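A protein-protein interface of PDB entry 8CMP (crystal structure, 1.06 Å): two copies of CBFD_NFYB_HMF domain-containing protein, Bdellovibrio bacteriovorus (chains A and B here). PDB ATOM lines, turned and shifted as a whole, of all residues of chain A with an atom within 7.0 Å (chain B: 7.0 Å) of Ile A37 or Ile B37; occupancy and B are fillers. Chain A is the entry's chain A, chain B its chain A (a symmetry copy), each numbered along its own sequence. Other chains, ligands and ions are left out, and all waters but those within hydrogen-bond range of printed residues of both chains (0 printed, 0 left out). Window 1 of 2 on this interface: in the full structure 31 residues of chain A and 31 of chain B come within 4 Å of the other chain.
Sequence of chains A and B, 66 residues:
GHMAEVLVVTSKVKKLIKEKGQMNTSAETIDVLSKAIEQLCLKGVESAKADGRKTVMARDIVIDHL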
ATOM      1  N   LEU A   7       6.958  -8.410  28.261  1.00  0.00           N
ATOM      2  CA  LEU A   7       6.225  -9.325  27.364  1.00  0.00           C
ATOM      3  C   LEU A   7       7.106  -9.936  26.294  1.00  0.00           C
ATOM      4  O   LEU A   7       6.627 -10.763  25.501  1.00  0.00           O
ATOM      5  CB  LEU A   7       5.047  -8.615  26.733  1.00  0.00           C
ATOM      6  CG  LEU A   7       3.980  -8.129  27.704  1.00  0.00           C
ATOM      7  CD1 LEU A   7       2.992  -7.231  27.025  1.00  0.00           C
ATOM      8  CD2 LEU A   7       3.362  -9.281  28.435  1.00  0.00           C
ATOM      9  N   VAL A   8       8.359  -9.491  26.189  1.00  0.00           N
ATOM     10  CA  VAL A   8       9.321 -10.088  25.270  1.00  0.00           C
ATOM     11  C   VAL A   8      10.280 -10.961  26.049  1.00  0.00           C
ATOM     12  O   VAL A   8      10.527 -10.728  27.222  1.00  0.00           O
ATOM     13  CB  VAL A   8      10.050  -9.064  24.418  1.00  0.00           C
ATOM     14  CG1 VAL A   8       9.042  -8.347  23.540  1.00  0.00           C
ATOM     15  CG2 VAL A   8      10.912  -8.138  25.238  1.00  0.00           C
ATOM     16  N   VAL A   9      10.858 -11.920  25.341  1.00  0.00           N
ATOM     17  CA  VAL A   9      11.851 -12.832  25.938  1.00  0.00           C
ATOM     18  C   VAL A   9      13.201 -12.125  25.813  1.00  0.00           C
ATOM     19  O   VAL A   9      13.854 -12.184  24.778  1.00  0.00           O
ATOM     20  CB  VAL A   9      11.863 -14.221  25.286  1.00  0.00           C
ATOM     21  CG1 VAL A   9      12.853 -15.124  26.029  1.00  0.00           C
ATOM     22  CG2 VAL A   9      10.479 -14.831  25.245  1.00  0.00           C
ATOM     23  N   VAL A  13      15.775 -11.804  22.536  1.00  0.00           N
ATOM     24  CA  VAL A  13      15.893 -10.537  21.786  1.00  0.00           C
ATOM     25  C   VAL A  13      17.360 -10.117  21.742  1.00  0.00           C
ATOM     26  O   VAL A  13      17.882  -9.758  20.696  1.00  0.00           O
ATOM     27  CB  VAL A  13      15.012  -9.463  22.435  1.00  0.00           C
ATOM     28  CG1 VAL A  13      15.405  -8.084  21.961  1.00  0.00           C
ATOM     29  CG2 VAL A  13      13.544  -9.798  22.205  1.00  0.00           C
ATOM     30  N   LEU A  16      19.288 -12.373  19.366  1.00  0.00           N
ATOM     31  CA  LEU A  16      18.994 -12.069  17.945  1.00  0.00           C
ATOM     32  C   LEU A  16      19.803 -10.823  17.498  1.00  0.00           C
ATOM     33  O   LEU A  16      20.468 -10.845  16.462  1.00  0.00           O
ATOM     34  CB  LEU A  16      17.495 -11.794  17.794  1.00  0.00           C
ATOM     35  CG  LEU A  16      17.033 -11.345  16.398  1.00  0.00           C
ATOM     36  CD1 LEU A  16      17.271 -12.430  15.376  1.00  0.00           C
ATOM     37  CD2 LEU A  16      15.585 -10.919  16.423  1.00  0.00           C
ATOM     38  N   ASP A  31      12.117  -2.355  26.844  1.00  0.00           N
ATOM     39  CA  ASP A  31      10.869  -1.717  27.299  1.00  0.00           C
ATOM     40  C   ASP A  31       9.993  -1.309  26.133  1.00  0.00           C
ATOM     41  O   ASP A  31       8.770  -1.540  26.184  1.00  0.00           O
ATOM     42  CB  ASP A  31      11.150  -0.512  28.165  1.00  0.00           C
ATOM     43  CG  ASP A  31      11.743  -0.829  29.495  1.00  0.00           C
ATOM     44  OD1 ASP A  31      11.520  -1.921  29.995  1.00  0.00           O
ATOM     45  OD2 ASP A  31      12.370   0.078  30.060  1.00  0.00           O
ATOM     46  N   VAL A  32      10.560  -0.723  25.097  1.00  0.00           N
ATOM     47  CA  VAL A  32       9.739  -0.310  23.939  1.00  0.00           C
ATOM     48  C   VAL A  32       9.147  -1.534  23.268  1.00  0.00           C
ATOM     49  O   VAL A  32       7.983  -1.492  22.845  1.00  0.00           O
ATOM     50  CB  VAL A  32      10.558   0.494  22.935  1.00  0.00           C
ATOM     51  CG1 VAL A  32       9.792   0.738  21.634  1.00  0.00           C
ATOM     52  CG2 VAL A  32      11.073   1.746  23.477  1.00  0.00           C
ATOM     53  N   LEU A  33       9.929  -2.591  23.105  1.00  0.00           N
ATOM     54  CA  LEU A  33       9.395  -3.812  22.475  1.00  0.00           C
ATOM     55  C   LEU A  33       8.252  -4.378  23.293  1.00  0.00           C
ATOM     56  O   LEU A  33       7.235  -4.801  22.728  1.00  0.00           O
ATOM     57  CB  LEU A  33      10.525  -4.816  22.320  1.00  0.00           C
ATOM     58  CG  LEU A  33      11.586  -4.443  21.283  1.00  0.00           C
ATOM     59  CD1 LEU A  33      12.767  -5.392  21.425  1.00  0.00           C
ATOM     60  CD2 LEU A  33      11.081  -4.460  19.856  1.00  0.00           C
ATOM     61  N   SER A  34       8.394  -4.414  24.603  1.00  0.00           N
ATOM     62  CA  SER A  34       7.328  -4.927  25.461  1.00  0.00           C
ATOM     63  C   SER A  34       6.074  -4.043  25.336  1.00  0.00           C
ATOM     64  O   SER A  34       4.959  -4.589  25.253  1.00  0.00           O
ATOM     65  CB  SER A  34       7.852  -4.992  26.871  1.00  0.00           C
ATOM     66  OG  SER A  34       6.926  -5.612  27.713  1.00  0.00           O
ATOM     67  N   LYS A  35       6.233  -2.739  25.333  1.00  0.00           N
ATOM     68  CA  LYS A  35       5.100  -1.835  25.185  1.00  0.00           C
ATOM     69  C   LYS A  35       4.436  -2.050  23.833  1.00  0.00           C
ATOM     70  O   LYS A  35       3.200  -1.948  23.721  1.00  0.00           O
ATOM     71  CB  LYS A  35       5.540  -0.386  25.382  1.00  0.00           C
ATOM     72  CG  LYS A  35       5.929  -0.012  26.799  1.00  0.00           C
ATOM     73  CD  LYS A  35       4.822   0.359  27.752  1.00  0.00           C
ATOM     74  CE  LYS A  35       5.388   0.898  29.069  1.00  0.00           C
ATOM     75  NZ  LYS A  35       4.403   0.839  30.166  1.00  0.00           N
ATOM     76  N   ALA A  36       5.233  -2.307  22.815  1.00  0.00           N
ATOM     77  CA  ALA A  36       4.659  -2.535  21.485  1.00  0.00           C
ATOM     78  C   ALA A  36       3.775  -3.803  21.513  1.00  0.00           C
ATOM     79  O   ALA A  36       2.679  -3.812  20.933  1.00  0.00           O
ATOM     80  CB  ALA A  36       5.755  -2.690  20.465  1.00  0.00           C
ATOM     81  N   ILE A  37       4.248  -4.853  22.148  1.00  0.00           N
ATOM     82  CA  ILE A  37       3.442  -6.083  22.273  1.00  0.00           C
ATOM     83  C   ILE A  37       2.172  -5.781  23.045  1.00  0.00           C
ATOM     84  O   ILE A  37       1.087  -6.220  22.627  1.00  0.00           O
ATOM     85  CB  ILE A  37       4.233  -7.213  22.944  1.00  0.00           C
ATOM     86  CG1 ILE A  37       5.402  -7.639  22.064  1.00  0.00           C
ATOM     87  CG2 ILE A  37       3.329  -8.398  23.247  1.00  0.00           C
ATOM     88  CD1 ILE A  37       4.957  -8.084  20.673  1.00  0.00           C
ATOM     89  N   GLU A  38       2.256  -5.033  24.117  1.00  0.00           N
ATOM     90  CA  GLU A  38       1.052  -4.731  24.899  1.00  0.00           C
ATOM     91  C   GLU A  38       0.055  -4.011  23.998  1.00  0.00           C
ATOM     92  O   GLU A  38      -1.162  -4.363  23.996  1.00  0.00           O
ATOM     93  CB  GLU A  38       1.424  -3.867  26.072  1.00  0.00           C
ATOM     94  CG  GLU A  38       0.278  -3.495  26.951  1.00  0.00           C
ATOM     95  CD  GLU A  38       0.648  -2.535  28.064  1.00  0.00           C
ATOM     96  OE1 GLU A  38       1.423  -1.628  27.827  1.00  0.00           O
ATOM     97  OE2 GLU A  38       0.126  -2.680  29.134  1.00  0.00           O
ATOM     98  N   GLN A  39       0.489  -3.003  23.239  1.00  0.00           N
ATOM     99  CA  GLN A  39      -0.432  -2.246  22.402  1.00  0.00           C
ATOM    100  C   GLN A  39      -1.010  -3.118  21.309  1.00  0.00           C
ATOM    101  O   GLN A  39      -2.209  -3.002  21.006  1.00  0.00           O
ATOM    102  CB  GLN A  39       0.315  -1.053  21.854  1.00  0.00           C
ATOM    103  CG  GLN A  39       0.569   0.001  22.936  1.00  0.00           C
ATOM    104  CD  GLN A  39      -0.704   0.417  23.672  1.00  0.00           C
ATOM    105  OE1 GLN A  39      -1.700   0.847  23.081  1.00  0.00           O
ATOM    106  NE2 GLN A  39      -0.723   0.234  24.989  1.00  0.00           N
ATOM    107  N   LEU A  40      -0.193  -3.972  20.683  1.00  0.00           N
ATOM    108  CA  LEU A  40      -0.720  -4.867  19.648  1.00  0.00           C
ATOM    109  C   LEU A  40      -1.772  -5.791  20.247  1.00  0.00           C
ATOM    110  O   LEU A  40      -2.789  -6.072  19.579  1.00  0.00           O
ATOM    111  CB  LEU A  40       0.405  -5.660  18.995  1.00  0.00           C
ATOM    112  CG  LEU A  40       1.339  -4.854  18.099  1.00  0.00           C
ATOM    113  CD1 LEU A  40       2.514  -5.708  17.698  1.00  0.00           C
ATOM    114  CD2 LEU A  40       0.610  -4.339  16.879  1.00  0.00           C
ATOM    115  N   CYS A  41      -1.534  -6.301  21.428  1.00  0.00           N
ATOM    116  CA  CYS A  41      -2.505  -7.199  22.066  1.00  0.00           C
ATOM    117  C   CYS A  41      -3.810  -6.477  22.362  1.00  0.00           C
ATOM    118  O   CYS A  41      -4.897  -7.027  22.116  1.00  0.00           O
ATOM    119  CB  CYS A  41      -1.937  -7.783  23.341  1.00  0.00           C
ATOM    120  SG  CYS A  41      -0.641  -9.011  23.083  1.00  0.00           S
ATOM    121  N   LEU A  42      -3.716  -5.271  22.904  1.00  0.00           N
ATOM    122  CA  LEU A  42      -4.936  -4.546  23.257  1.00  0.00           C
ATOM    123  C   LEU A  42      -5.695  -4.162  21.987  1.00  0.00           C
ATOM    124  O   LEU A  42      -6.936  -4.232  21.984  1.00  0.00           O
ATOM    125  CB  LEU A  42      -4.596  -3.333  24.113  1.00  0.00           C
ATOM    126  CG  LEU A  42      -4.055  -3.626  25.492  1.00  0.00           C
ATOM    127  CD1 LEU A  42      -3.563  -2.345  26.155  1.00  0.00           C
ATOM    128  CD2 LEU A  42      -5.095  -4.316  26.351  1.00  0.00           C
ATOM    129  N   LYS A  43      -5.026  -3.749  20.934  1.00  0.00           N
ATOM    130  CA  LYS A  43      -5.713  -3.465  19.672  1.00  0.00           C
ATOM    131  C   LYS A  43      -6.307  -4.750  19.127  1.00  0.00           C
ATOM    132  O   LYS A  43      -7.389  -4.729  18.501  1.00  0.00           O
ATOM    133  CB  LYS A  43      -4.756  -2.806  18.692  1.00  0.00           C
ATOM    134  CG  LYS A  43      -4.402  -1.376  19.102  1.00  0.00           C
ATOM    135  CD  LYS A  43      -3.486  -0.645  18.144  1.00  0.00           C
ATOM    136  CE  LYS A  43      -3.043   0.696  18.702  1.00  0.00           C
ATOM    137  NZ  LYS A  43      -2.297   1.508  17.715  1.00  0.00           N
ATOM    138  N   ILE A  61      -4.088  -8.674  14.641  1.00  0.00           N
ATOM    139  CA  ILE A  61      -2.784  -8.044  15.007  1.00  0.00           C
ATOM    140  C   ILE A  61      -2.355  -7.279  13.790  1.00  0.00           C
ATOM    141  O   ILE A  61      -1.861  -7.865  12.821  1.00  0.00           O
ATOM    142  CB  ILE A  61      -1.755  -9.089  15.401  1.00  0.00           C
ATOM    143  CG1 ILE A  61      -2.247  -9.986  16.534  1.00  0.00           C
ATOM    144  CG2 ILE A  61      -0.428  -8.460  15.776  1.00  0.00           C
ATOM    145  CD1 ILE A  61      -2.665  -9.258  17.774  1.00  0.00           C
ATOM    146  N   LEU B   7       9.718 -15.099  20.426  1.00  0.00           N
ATOM    147  CA  LEU B   7      10.336 -13.912  21.050  1.00  0.00           C
ATOM    148  C   LEU B   7       9.420 -13.221  22.040  1.00  0.00           C
ATOM    149  O   LEU B   7       9.832 -12.236  22.675  1.00  0.00           O
ATOM    150  CB  LEU B   7      10.796 -12.936  19.989  1.00  0.00           C
ATOM    151  CG  LEU B   7      11.876 -13.454  19.050  1.00  0.00           C
ATOM    152  CD1 LEU B   7      12.086 -12.524  17.894  1.00  0.00           C
ATOM    153  CD2 LEU B   7      13.126 -13.785  19.807  1.00  0.00           C
ATOM    154  N   VAL B   8       8.161 -13.650  22.129  1.00  0.00           N
ATOM    155  CA  VAL B   8       7.231 -13.131  23.125  1.00  0.00           C
ATOM    156  C   VAL B   8       7.075 -14.142  24.238  1.00  0.00           C
ATOM    157  O   VAL B   8       7.236 -15.335  24.028  1.00  0.00           O
ATOM    158  CB  VAL B   8       5.892 -12.720  22.538  1.00  0.00           C
ATOM    159  CG1 VAL B   8       6.111 -11.585  21.557  1.00  0.00           C
ATOM    160  CG2 VAL B   8       5.132 -13.887  21.960  1.00  0.00           C
ATOM    161  N   VAL B   9       6.689 -13.635  25.399  1.00  0.00           N
ATOM    162  CA  VAL B   9       6.448 -14.491  26.576  1.00  0.00           C
ATOM    163  C   VAL B   9       4.998 -14.962  26.464  1.00  0.00           C
ATOM    164  O   VAL B   9       4.071 -14.262  26.856  1.00  0.00           O
ATOM    165  CB  VAL B   9       6.724 -13.778  27.907  1.00  0.00           C
ATOM    166  CG1 VAL B   9       6.539 -14.767  29.062  1.00  0.00           C
ATOM    167  CG2 VAL B   9       8.099 -13.149  27.930  1.00  0.00           C
ATOM    168  N   VAL B  13       1.445 -12.985  27.436  1.00  0.00           N
ATOM    169  CA  VAL B  13       0.562 -12.452  26.379  1.00  0.00           C
ATOM    170  C   VAL B  13      -0.843 -13.019  26.570  1.00  0.00           C
ATOM    171  O   VAL B  13      -1.827 -12.292  26.527  1.00  0.00           O
ATOM    172  CB  VAL B  13       1.132 -12.797  24.998  1.00  0.00           C
ATOM    173  CG1 VAL B  13       0.082 -12.634  23.925  1.00  0.00           C
ATOM    174  CG2 VAL B  13       2.398 -11.987  24.750  1.00  0.00           C
ATOM    175  N   LEU B  16      -2.502 -11.395  29.580  1.00  0.00           N
ATOM    176  CA  LEU B  16      -2.930 -10.003  29.300  1.00  0.00           C
ATOM    177  C   LEU B  16      -4.264 -10.015  28.508  1.00  0.00           C
ATOM    178  O   LEU B  16      -5.215  -9.322  28.871  1.00  0.00           O
ATOM    179  CB  LEU B  16      -1.845  -9.305  28.474  1.00  0.00           C
ATOM    180  CG  LEU B  16      -2.179  -7.884  27.993  1.00  0.00           C
ATOM    181  CD1 LEU B  16      -2.354  -6.945  29.162  1.00  0.00           C
ATOM    182  CD2 LEU B  16      -1.126  -7.380  27.035  1.00  0.00           C
ATOM    183  N   ASP B  31       2.504 -16.326  16.998  1.00  0.00           N
ATOM    184  CA  ASP B  31       3.476 -16.313  15.890  1.00  0.00           C
ATOM    185  C   ASP B  31       3.593 -14.938  15.267  1.00  0.00           C
ATOM    186  O   ASP B  31       4.724 -14.490  14.997  1.00  0.00           O
ATOM    187  CB  ASP B  31       3.110 -17.321  14.826  1.00  0.00           C
ATOM    188  CG  ASP B  31       3.258 -18.745  15.242  1.00  0.00           C
ATOM    189  OD1 ASP B  31       4.064 -19.022  16.116  1.00  0.00           O
ATOM    190  OD2 ASP B  31       2.602 -19.584  14.610  1.00  0.00           O
ATOM    191  N   VAL B  32       2.488 -14.259  15.033  1.00  0.00           N
ATOM    192  CA  VAL B  32       2.560 -12.913  14.425  1.00  0.00           C
ATOM    193  C   VAL B  32       3.268 -11.962  15.370  1.00  0.00           C
ATOM    194  O   VAL B  32       4.057 -11.125  14.911  1.00  0.00           O
ATOM    195  CB  VAL B  32       1.171 -12.380  14.087  1.00  0.00           C
ATOM    196  CG1 VAL B  32       1.208 -10.910  13.667  1.00  0.00           C
ATOM    197  CG2 VAL B  32       0.466 -13.186  13.097  1.00  0.00           C
ATOM    198  N   LEU B  33       2.963 -12.026  16.657  1.00  0.00           N
ATOM    199  CA  LEU B  33       3.638 -11.135  17.619  1.00  0.00           C
ATOM    200  C   LEU B  33       5.131 -11.392  17.628  1.00  0.00           C
ATOM    201  O   LEU B  33       5.923 -10.442  17.663  1.00  0.00           O
ATOM    202  CB  LEU B  33       3.024 -11.347  18.993  1.00  0.00           C
ATOM    203  CG  LEU B  33       1.589 -10.840  19.148  1.00  0.00           C
ATOM    204  CD1 LEU B  33       1.029 -11.347  20.468  1.00  0.00           C
ATOM    205  CD2 LEU B  33       1.460  -9.333  19.080  1.00  0.00           C
ATOM    206  N   SER B  34       5.538 -12.646  17.612  1.00  0.00           N
ATOM    207  CA  SER B  34       6.962 -12.974  17.598  1.00  0.00           C
ATOM    208  C   SER B  34       7.616 -12.448  16.308  1.00  0.00           C
ATOM    209  O   SER B  34       8.726 -11.891  16.380  1.00  0.00           O
ATOM    210  CB  SER B  34       7.100 -14.465  17.750  1.00  0.00           C
ATOM    211  OG  SER B  34       8.442 -14.824  17.890  1.00  0.00           O
ATOM    212  N   LYS B  35       6.974 -12.619  15.174  1.00  0.00           N
ATOM    213  CA  LYS B  35       7.510 -12.121  13.914  1.00  0.00           C
ATOM    214  C   LYS B  35       7.620 -10.604  13.960  1.00  0.00           C
ATOM    215  O   LYS B  35       8.568 -10.029  13.392  1.00  0.00           O
ATOM    216  CB  LYS B  35       6.657 -12.598  12.742  1.00  0.00           C
ATOM    217  CG  LYS B  35       6.740 -14.080  12.438  1.00  0.00           C
ATOM    218  CD  LYS B  35       7.891 -14.556  11.589  1.00  0.00           C
ATOM    219  CE  LYS B  35       7.723 -16.030  11.211  1.00  0.00           C
ATOM    220  NZ  LYS B  35       8.996 -16.648  10.794  1.00  0.00           N
ATOM    221  N   ALA B  36       6.657  -9.958  14.587  1.00  0.00           N
ATOM    222  CA  ALA B  36       6.706  -8.495  14.678  1.00  0.00           C
ATOM    223  C   ALA B  36       7.948  -8.068  15.494  1.00  0.00           C
ATOM    224  O   ALA B  36       8.639  -7.109  15.120  1.00  0.00           O
ATOM    225  CB  ALA B  36       5.454  -7.973  15.329  1.00  0.00           C
ATOM    226  N   ILE B  37       8.210  -8.744  16.591  1.00  0.00           N
ATOM    227  CA  ILE B  37       9.410  -8.439  17.395  1.00  0.00           C
ATOM    228  C   ILE B  37      10.653  -8.679  16.561  1.00  0.00           C
ATOM    229  O   ILE B  37      11.566  -7.836  16.573  1.00  0.00           O
ATOM    230  CB  ILE B  37       9.451  -9.265  18.686  1.00  0.00           C
ATOM    231  CG1 ILE B  37       8.297  -8.876  19.604  1.00  0.00           C
ATOM    232  CG2 ILE B  37      10.784  -9.089  19.397  1.00  0.00           C
ATOM    233  CD1 ILE B  37       8.299  -7.389  19.949  1.00  0.00           C
ATOM    234  N   GLU B  38      10.711  -9.760  15.822  1.00  0.00           N
ATOM    235  CA  GLU B  38      11.903 -10.035  15.013  1.00  0.00           C
ATOM    236  C   GLU B  38      12.103  -8.883  14.035  1.00  0.00           C
ATOM    237  O   GLU B  38      13.255  -8.376  13.883  1.00  0.00           O
ATOM    238  CB  GLU B  38      11.714 -11.329  14.272  1.00  0.00           C
ATOM    239  CG  GLU B  38      12.869 -11.723  13.414  1.00  0.00           C
ATOM    240  CD  GLU B  38      12.621 -12.969  12.589  1.00  0.00           C
ATOM    241  OE1 GLU B  38      11.530 -13.132  12.079  1.00  0.00           O
ATOM    242  OE2 GLU B  38      13.531 -13.736  12.434  1.00  0.00           O
ATOM    243  N   GLN B  39      11.053  -8.442  13.341  1.00  0.00           N
ATOM    244  CA  GLN B  39      11.200  -7.381  12.353  1.00  0.00           C
ATOM    245  C   GLN B  39      11.595  -6.079  13.015  1.00  0.00           C
ATOM    246  O   GLN B  39      12.432  -5.345  12.463  1.00  0.00           O
ATOM    247  CB  GLN B  39       9.899  -7.271  11.594  1.00  0.00           C
ATOM    248  CG  GLN B  39       9.700  -8.453  10.640  1.00  0.00           C
ATOM    249  CD  GLN B  39      10.887  -8.669   9.703  1.00  0.00           C
ATOM    250  OE1 GLN B  39      11.320  -7.777   8.967  1.00  0.00           O
ATOM    251  NE2 GLN B  39      11.488  -9.854   9.759  1.00  0.00           N
ATOM    252  N   LEU B  40      11.001  -5.748  14.166  1.00  0.00           N
ATOM    253  CA  LEU B  40      11.385  -4.518  14.863  1.00  0.00           C
ATOM    254  C   LEU B  40      12.856  -4.578  15.253  1.00  0.00           C
ATOM    255  O   LEU B  40      13.553  -3.546  15.166  1.00  0.00           O
ATOM    256  CB  LEU B  40      10.500  -4.288  16.081  1.00  0.00           C
ATOM    257  CG  LEU B  40       9.057  -3.898  15.778  1.00  0.00           C
ATOM    258  CD1 LEU B  40       8.252  -3.914  17.052  1.00  0.00           C
ATOM    259  CD2 LEU B  40       8.989  -2.540  15.119  1.00  0.00           C
ATOM    260  N   CYS B  41      13.317  -5.711  15.720  1.00  0.00           N
ATOM    261  CA  CYS B  41      14.725  -5.840  16.114  1.00  0.00           C
ATOM    262  C   CYS B  41      15.649  -5.666  14.918  1.00  0.00           C
ATOM    263  O   CYS B  41      16.674  -4.970  15.018  1.00  0.00           O
ATOM    264  CB  CYS B  41      14.976  -7.180  16.770  1.00  0.00           C
ATOM    265  SG  CYS B  41      14.271  -7.342  18.422  1.00  0.00           S
ATOM    266  N   LEU B  42      15.314  -6.304  13.806  1.00  0.00           N
ATOM    267  CA  LEU B  42      16.187  -6.215  12.636  1.00  0.00           C
ATOM    268  C   LEU B  42      16.175  -4.788  12.090  1.00  0.00           C
ATOM    269  O   LEU B  42      17.237  -4.297  11.669  1.00  0.00           O
ATOM    270  CB  LEU B  42      15.766  -7.237  11.589  1.00  0.00           C
ATOM    271  CG  LEU B  42      15.966  -8.687  11.959  1.00  0.00           C
ATOM    272  CD1 LEU B  42      15.317  -9.598  10.924  1.00  0.00           C
ATOM    273  CD2 LEU B  42      17.438  -9.011  12.117  1.00  0.00           C
ATOM    274  N   LYS B  43      15.046  -4.119  12.055  1.00  0.00           N
ATOM    275  CA  LYS B  43      15.016  -2.718  11.627  1.00  0.00           C
ATOM    276  C   LYS B  43      15.798  -1.876  12.617  1.00  0.00           C
ATOM    277  O   LYS B  43      16.449  -0.884  12.225  1.00  0.00           O
ATOM    278  CB  LYS B  43      13.579  -2.248  11.474  1.00  0.00           C
ATOM    279  CG  LYS B  43      12.887  -2.884  10.268  1.00  0.00           C
ATOM    280  CD  LYS B  43      11.465  -2.426  10.031  1.00  0.00           C
ATOM    281  CE  LYS B  43      10.791  -3.225   8.929  1.00  0.00           C
ATOM    282  NZ  LYS B  43       9.467  -2.680   8.554  1.00  0.00           N
ATOM    283  N   ILE B  61      13.722   1.713  17.438  1.00  0.00           N
ATOM    284  CA  ILE B  61      12.532   0.816  17.341  1.00  0.00           C
ATOM    285  C   ILE B  61      11.401   1.699  16.903  1.00  0.00           C
ATOM    286  O   ILE B  61      10.839   2.447  17.710  1.00  0.00           O
ATOM    287  CB  ILE B  61      12.233   0.143  18.670  1.00  0.00           C
ATOM    288  CG1 ILE B  61      13.434  -0.626  19.210  1.00  0.00           C
ATOM    289  CG2 ILE B  61      11.028  -0.770  18.581  1.00  0.00           C
ATOM    290  CD1 ILE B  61      13.984  -1.664  18.281  1.00  0.00           C
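The backbone carbonyl oxygen of Leu B7 sits at hydrogen-bond distance from the backbone NH of Val A9. N of Val B9 lies within hydrogen-bond range of O of Leu A7, 2.9 Å away.
O of Ile B37 is in hydrogen-bond range of SG of Cys B41, at 3.3 Å. The side-chain sulfur (SG) of Cys A41 lies within hydrogen-bond range of the backbone carbonyl oxygen (O) of Ile A37 (3.3 Å). OG of Ser B34 is in hydrogen-bond range of N of Leu B7. OG of Ser A34 is in hydrogen-bond range of N of Leu A7, 2.9 Å away.
Among the printed residues, merely in contact across the chains: Val A8 with Leu B7, Leu A7 with Val B8, Ile A37 with Ile B37, Val A9 with Val B8, Val A8 with Val B9, Val A32 with Ile B61, Ile A61 with Val B32, Cys A41 with Val B13, Val A13 with Cys B41, Val A8 with Ile B37, Ile A37 with Val B8, Cys A41 with Leu B16, Leu A16 with Cys B41, Leu A40 with Leu B33, Leu A33 with Leu B40, Leu A33 with Cys B41, Cys A41 with Leu B33, Ile A61 with Leu B33, Leu A33 with Ile B61, Leu A33 with Ile B37, Ile A37 with Leu B33 and Val A9 with Val B9.
Printed residues of chain B within 4 Å of Val A13: Cys B41. Asp A31 touches none of the printed residues of chain B. Of the printed residues of chain B, Ile A37 touches Val B8 (3.8 Å), Leu B33 (3.9 Å) and Ile B37 (3.5 Å). Of the printed residues of chain A, Leu B16 touches Cys A41 (3.8 Å). Of the printed residues of chain A, Ile B37 touches Val A8 (3.8 Å), Leu A33 (3.9 Å) and Ile A37 (3.5 Å). Lys B43 touches none of the printed residues of chain A. The nearest printed residue of chain B that does not touch Val A9 is Ile B37 (6.6 Å).
Of the 19 printed residues of chain B, 11 touch a printed residue of chain A. Hydrophobic or aromatic side chains of chain B that line the printed part of chain A: Val B8, Val B9, Val B13, Leu B16, Val B32, Leu B33, Ile B37, Leu B40 and Ile B61. Along chain B the printed residues that touch a printed residue of chain A span positions 7 to 61. Hydrophobic or aromatic side chains of chain A within 4 Å of the printed part of chain B: Val A8, Val A9, Val A13, Leu A16, Val A32, Leu A33, Ile A37, Leu A40 and Ile A61. Among the printed residues, no Asp or Glu carboxylate lies within 4 Å of a Lys or Arg side-chain nitrogen of the other chain.
Val A8 touches Val B9, and with the chains exchanged Val A9 touches Val B8. Val A9 touches its own counterpart, Val B9. Val A32 touches Ile B61, and with the chains exchanged Ile A61 touches Val B32. Leu A33 touches Ile B61, and with the chains exchanged Ile A61 touches Leu B33. Positions printed for both chains: 7, 8, 9, 13, 16, 31, 32, 33, 34, 35, 36, 37, 38, 39, 40, 41, 42, 43 and 61. Of the 24 pairs that touch across the chains among the printed residues, 24 have their exchanged pair printed and touching as well.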
